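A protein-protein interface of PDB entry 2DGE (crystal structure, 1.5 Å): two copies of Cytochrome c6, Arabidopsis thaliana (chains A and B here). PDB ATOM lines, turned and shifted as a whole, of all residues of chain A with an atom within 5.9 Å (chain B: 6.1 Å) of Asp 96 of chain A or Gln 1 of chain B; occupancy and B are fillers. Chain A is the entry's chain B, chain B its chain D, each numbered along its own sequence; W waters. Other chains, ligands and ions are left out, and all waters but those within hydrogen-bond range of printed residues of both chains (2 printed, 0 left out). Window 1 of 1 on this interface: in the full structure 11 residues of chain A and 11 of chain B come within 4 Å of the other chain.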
ATOM      1  N   THR A  35      20.191  -9.511  18.308  1.00  0.00           N
ATOM      2  CA  THR A  35      20.028 -10.651  19.210  1.00  0.00           C
ATOM      3  C   THR A  35      18.577 -11.099  19.374  1.00  0.00           C
ATOM      4  O   THR A  35      18.280 -12.290  19.331  1.00  0.00           O
ATOM      5  CB  THR A  35      20.643 -10.303  20.581  1.00  0.00           C
ATOM      6  OG1 THR A  35      22.063 -10.166  20.422  1.00  0.00           O
ATOM      7  CG2 THR A  35      20.515 -11.473  21.555  1.00  0.00           C
ATOM      8  N   GLU A  46      26.339 -19.583  16.706  1.00  0.00           N
ATOM      9  CA  GLU A  46      27.263 -19.347  15.620  1.00  0.00           C
ATOM     10  C   GLU A  46      27.163 -20.410  14.513  1.00  0.00           C
ATOM     11  O   GLU A  46      27.262 -20.096  13.324  1.00  0.00           O
ATOM     12  CB  GLU A  46      28.676 -19.301  16.175  1.00  0.00           C
ATOM     13  CG  GLU A  46      29.589 -18.442  15.351  1.00  0.00           C
ATOM     14  CD  GLU A  46      30.834 -18.058  16.098  1.00  0.00           C
ATOM     15  OE1 GLU A  46      30.784 -17.983  17.347  1.00  0.00           O
ATOM     16  OE2 GLU A  46      31.843 -17.831  15.421  1.00  0.00           O
ATOM     17  N   VAL A  91      28.805 -11.789  12.603  1.00  0.00           N
ATOM     18  CA  VAL A  91      27.398 -11.595  12.967  1.00  0.00           C
ATOM     19  C   VAL A  91      27.183 -11.926  14.450  1.00  0.00           C
ATOM     20  O   VAL A  91      26.527 -11.159  15.171  1.00  0.00           O
ATOM     21  CB  VAL A  91      26.442 -12.428  12.057  1.00  0.00           C
ATOM     22  CG1 VAL A  91      25.001 -12.338  12.542  1.00  0.00           C
ATOM     23  CG2 VAL A  91      26.524 -11.957  10.611  1.00  0.00           C
ATOM     24  N   LYS A  92      27.722 -13.058  14.910  1.00  0.00           N
ATOM     25  CA  LYS A  92      27.551 -13.450  16.303  1.00  0.00           C
ATOM     26  C   LYS A  92      28.131 -12.384  17.238  1.00  0.00           C
ATOM     27  O   LYS A  92      27.480 -11.992  18.219  1.00  0.00           O
ATOM     28  CB  LYS A  92      28.211 -14.818  16.571  1.00  0.00           C
ATOM     29  CG  LYS A  92      28.063 -15.312  18.023  1.00  0.00           C
ATOM     30  CD  LYS A  92      26.618 -15.619  18.356  1.00  0.00           C
ATOM     31  CE  LYS A  92      26.552 -16.464  19.616  1.00  0.00           C
ATOM     32  NZ  LYS A  92      26.300 -15.610  20.784  1.00  0.00           N
ATOM     33  N   PHE A  93      29.353 -11.929  16.948  1.00  0.00           N
ATOM     34  CA  PHE A  93      29.973 -10.881  17.762  1.00  0.00           C
ATOM     35  C   PHE A  93      29.160  -9.592  17.765  1.00  0.00           C
ATOM     36  O   PHE A  93      28.865  -9.032  18.824  1.00  0.00           O
ATOM     37  CB  PHE A  93      31.375 -10.581  17.276  1.00  0.00           C
ATOM     38  CG  PHE A  93      32.095  -9.619  18.142  1.00  0.00           C
ATOM     39  CD1 PHE A  93      32.464  -9.979  19.436  1.00  0.00           C
ATOM     40  CD2 PHE A  93      32.371  -8.339  17.680  1.00  0.00           C
ATOM     41  CE1 PHE A  93      33.133  -9.072  20.252  1.00  0.00           C
ATOM     42  CE2 PHE A  93      33.040  -7.431  18.487  1.00  0.00           C
ATOM     43  CZ  PHE A  93      33.421  -7.807  19.774  1.00  0.00           C
ATOM     44  N   GLN A  94      28.823  -9.114  16.578  1.00  0.00           N
ATOM     45  CA  GLN A  94      28.083  -7.863  16.460  1.00  0.00           C
ATOM     46  C   GLN A  94      26.728  -7.952  17.162  1.00  0.00           C
ATOM     47  O   GLN A  94      26.349  -7.040  17.896  1.00  0.00           O
ATOM     48  CB  GLN A  94      27.917  -7.463  14.998  1.00  0.00           C
ATOM     49  CG  GLN A  94      29.202  -6.911  14.375  1.00  0.00           C
ATOM     50  CD  GLN A  94      29.669  -5.612  15.035  1.00  0.00           C
ATOM     51  OE1 GLN A  94      30.513  -5.624  15.942  1.00  0.00           O
ATOM     52  NE2 GLN A  94      29.122  -4.502  14.583  1.00  0.00           N
ATOM     53  N   ALA A  95      26.017  -9.058  16.967  1.00  0.00           N
ATOM     54  CA  ALA A  95      24.768  -9.272  17.709  1.00  0.00           C
ATOM     55  C   ALA A  95      24.986  -9.227  19.229  1.00  0.00           C
ATOM     56  O   ALA A  95      24.261  -8.518  19.952  1.00  0.00           O
ATOM     57  CB  ALA A  95      24.127 -10.573  17.300  1.00  0.00           C
ATOM     58  N   ASP A  96      25.999  -9.945  19.717  1.00  0.00           N
ATOM     59  CA  ASP A  96      26.297  -9.966  21.154  1.00  0.00           C
ATOM     60  C   ASP A  96      26.571  -8.557  21.695  1.00  0.00           C
ATOM     61  O   ASP A  96      26.184  -8.215  22.841  1.00  0.00           O
ATOM     62  CB  ASP A  96      27.512 -10.860  21.437  1.00  0.00           C
ATOM     63  CG  ASP A  96      27.194 -12.340  21.348  1.00  0.00           C
ATOM     64  OD1 ASP A  96      28.160 -13.143  21.370  1.00  0.00           O
ATOM     65  OD2 ASP A  96      26.038 -12.809  21.261  1.00  0.00           O
ATOM     66  N   GLN A  97      27.224  -7.745  20.872  1.00  0.00           N
ATOM     67  CA  GLN A  97      27.666  -6.411  21.259  1.00  0.00           C
ATOM     68  C   GLN A  97      26.628  -5.337  20.945  1.00  0.00           C
ATOM     69  O   GLN A  97      26.835  -4.172  21.257  1.00  0.00           O
ATOM     70  CB  GLN A  97      29.001  -6.063  20.593  1.00  0.00           C
ATOM     71  CG  GLN A  97      30.177  -6.967  20.962  1.00  0.00           C
ATOM     72  CD  GLN A  97      30.652  -6.799  22.400  1.00  0.00           C
ATOM     73  OE1 GLN A  97      31.255  -5.783  22.746  1.00  0.00           O
ATOM     74  NE2 GLN A  97      30.393  -7.798  23.233  1.00  0.00           N
ATOM     75  N   GLY A  98      25.518  -5.717  20.318  1.00  0.00           N
ATOM     76  CA  GLY A  98      24.474  -4.761  19.985  1.00  0.00           C
ATOM     77  C   GLY A  98      24.794  -3.864  18.805  1.00  0.00           C
ATOM     78  O   GLY A  98      24.335  -2.721  18.752  1.00  0.00           O
ATOM     79  N   TRP A  99      25.586  -4.371  17.860  1.00  0.00           N
ATOM     80  CA  TRP A  99      25.927  -3.654  16.635  1.00  0.00           C
ATOM     81  C   TRP A  99      26.556  -2.263  16.855  1.00  0.00           C
ATOM     82  O   TRP A  99      26.047  -1.244  16.359  1.00  0.00           O
ATOM     83  CB  TRP A  99      24.721  -3.653  15.655  1.00  0.00           C
ATOM     84  CG  TRP A  99      24.539  -5.022  15.059  1.00  0.00           C
ATOM     85  CD1 TRP A  99      23.841  -6.067  15.588  1.00  0.00           C
ATOM     86  CD2 TRP A  99      25.123  -5.507  13.845  1.00  0.00           C
ATOM     87  NE1 TRP A  99      23.942  -7.168  14.774  1.00  0.00           N
ATOM     88  CE2 TRP A  99      24.732  -6.853  13.702  1.00  0.00           C
ATOM     89  CE3 TRP A  99      25.957  -4.943  12.870  1.00  0.00           C
ATOM     90  CZ2 TRP A  99      25.129  -7.638  12.616  1.00  0.00           C
ATOM     91  CZ3 TRP A  99      26.336  -5.719  11.774  1.00  0.00           C
ATOM     92  CH2 TRP A  99      25.919  -7.048  11.660  1.00  0.00           C
ATOM     93  N   GLN B   1      28.990 -14.846  23.547  1.00  0.00           N
ATOM     94  CA  GLN B   1      30.387 -14.801  23.013  1.00  0.00           C
ATOM     95  C   GLN B   1      30.607 -15.762  21.843  1.00  0.00           C
ATOM     96  O   GLN B   1      29.908 -16.759  21.688  1.00  0.00           O
ATOM     97  CB  GLN B   1      31.404 -15.046  24.127  1.00  0.00           C
ATOM     98  CG  GLN B   1      31.806 -16.491  24.296  1.00  0.00           C
ATOM     99  CD  GLN B   1      32.035 -16.880  25.737  1.00  0.00           C
ATOM    100  OE1 GLN B   1      33.178 -16.924  26.199  1.00  0.00           O
ATOM    101  NE2 GLN B   1      30.954 -17.191  26.448  1.00  0.00           N
ATOM    102  N   THR B   2      31.596 -15.452  21.019  1.00  0.00           N
ATOM    103  CA  THR B   2      31.903 -16.284  19.867  1.00  0.00           C
ATOM    104  C   THR B   2      32.677 -17.532  20.262  1.00  0.00           C
ATOM    105  O   THR B   2      33.220 -17.611  21.367  1.00  0.00           O
ATOM    106  CB  THR B   2      32.736 -15.504  18.859  1.00  0.00           C
ATOM    107  OG1 THR B   2      33.977 -15.139  19.477  1.00  0.00           O
ATOM    108  CG2 THR B   2      32.067 -14.167  18.499  1.00  0.00           C
ATOM    109  N   LEU B   3      32.754 -18.475  19.325  1.00  0.00           N
ATOM    110  CA  LEU B   3      33.548 -19.679  19.495  1.00  0.00           C
ATOM    111  C   LEU B   3      35.012 -19.309  19.724  1.00  0.00           C
ATOM    112  O   LEU B   3      35.666 -19.901  20.584  1.00  0.00           O
ATOM    113  CB  LEU B   3      33.450 -20.560  18.243  1.00  0.00           C
ATOM    114  CG  LEU B   3      32.026 -21.038  17.964  1.00  0.00           C
ATOM    115  CD1 LEU B   3      31.868 -21.660  16.576  1.00  0.00           C
ATOM    116  CD2 LEU B   3      31.549 -22.103  18.950  1.00  0.00           C
ATOM    117  N   ILE B   5      36.314 -16.541  20.992  1.00  0.00           N
ATOM    118  CA  ILE B   5      36.509 -16.000  22.337  1.00  0.00           C
ATOM    119  C   ILE B   5      36.463 -17.120  23.372  1.00  0.00           C
ATOM    120  O   ILE B   5      37.253 -17.135  24.297  1.00  0.00           O
ATOM    121  CB  ILE B   5      35.458 -14.924  22.677  1.00  0.00           C
ATOM    122  CG1 ILE B   5      35.704 -13.658  21.862  1.00  0.00           C
ATOM    123  CG2 ILE B   5      35.502 -14.570  24.182  1.00  0.00           C
ATOM    124  CD1 ILE B   5      34.474 -12.702  21.824  1.00  0.00           C
ATOM    125  N   GLN B   6      35.515 -18.039  23.229  1.00  0.00           N
ATOM    126  CA  GLN B   6      35.395 -19.147  24.174  1.00  0.00           C
ATOM    127  C   GLN B   6      36.678 -19.964  24.198  1.00  0.00           C
ATOM    128  O   GLN B   6      37.188 -20.297  25.275  1.00  0.00           O
ATOM    129  CB  GLN B   6      34.236 -20.053  23.787  1.00  0.00           C
ATOM    130  CG  GLN B   6      32.892 -19.564  24.232  1.00  0.00           C
ATOM    131  CD  GLN B   6      31.764 -20.433  23.727  1.00  0.00           C
ATOM    132  OE1 GLN B   6      31.903 -21.657  23.639  1.00  0.00           O
ATOM    133  NE2 GLN B   6      30.637 -19.809  23.397  1.00  0.00           N
ATOM    134  N   ALA B   9      39.560 -18.000  25.737  1.00  0.00           N
ATOM    135  CA  ALA B   9      39.459 -17.973  27.204  1.00  0.00           C
ATOM    136  C   ALA B   9      39.919 -19.273  27.837  1.00  0.00           C
ATOM    137  O   ALA B   9      40.591 -19.255  28.883  1.00  0.00           O
ATOM    138  CB  ALA B   9      38.042 -17.638  27.640  1.00  0.00           C
HETATM  139  O   HOH W   1      30.946 -12.109  21.384  1.00  0.00           O
HETATM  140  O   HOH W   2      29.335 -18.754  19.655  1.00  0.00           O
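The side-chain carboxylate (OE1) of Glu 46 of chain A sits at hydrogen-bond distance from the backbone NH (N) of Leu 3 of chain B, 2.8 Å away. OD1 of Asp 96 of chain A is in hydrogen-bond range of N of Gln 1 of chain B (2.9 Å).
The side-chain amino group of Lys 92 of chain A lies within salt-bridge range of the side-chain carboxylate of Asp 96 of chain A (2.9 Å). The side-chain hydroxyl (OG1) of Thr 2 of chain B sits at hydrogen-bond distance from the backbone NH (N) of Ile 5 of chain B (3.1 Å).
Among the printed residues, pairs that only touch across the chains: Glu 46 of chain A with Thr 2 of chain B, Phe 93 of chain A with Thr 2 of chain B and Lys 92 of chain A with Gln 1 of chain B.
Of the printed residues of chain B, Asp 96 of chain A touches Gln 1 (2.9 Å). Printed residues of chain B within 4 Å of Phe 93 of chain A: Thr 2. Printed residues of chain A within 4 Å of Leu 3 of chain B: Glu 46. The nearest residue of chain B that does not touch Asp 96 of chain A is Thr 2 of chain B (4.2 Å). The nearest residue of chain A that does not touch Gln 1 of chain B is Glu 46 of chain A (4.6 Å).
Printed residues of chain A that touch a printed residue of chain B: Glu 46, Lys 92, Phe 93 and Asp 96. Printed residues of chain B that touch a printed residue of chain A: Gln 1, Thr 2 and Leu 3. Among the printed residues, 5 pairs touch across the chains. Among the printed residues, no Asp or Glu carboxylate lies within 4 Å of a Lys or Arg side-chain nitrogen of the other chain.
No position is printed for both chains.
Water W2 lies within hydrogen-bond range of the side-chain carboxylate of Glu 46 of chain A, the backbone carbonyl oxygen of Gln 1 of chain B and the backbone NH of Leu 3 of chain B. Water W1 bridges the side-chain carboxylate (OD1) of Asp 96 of chain A (3.0 Å) and the backbone NH (N) of Thr 2 of chain B (3.4 Å).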
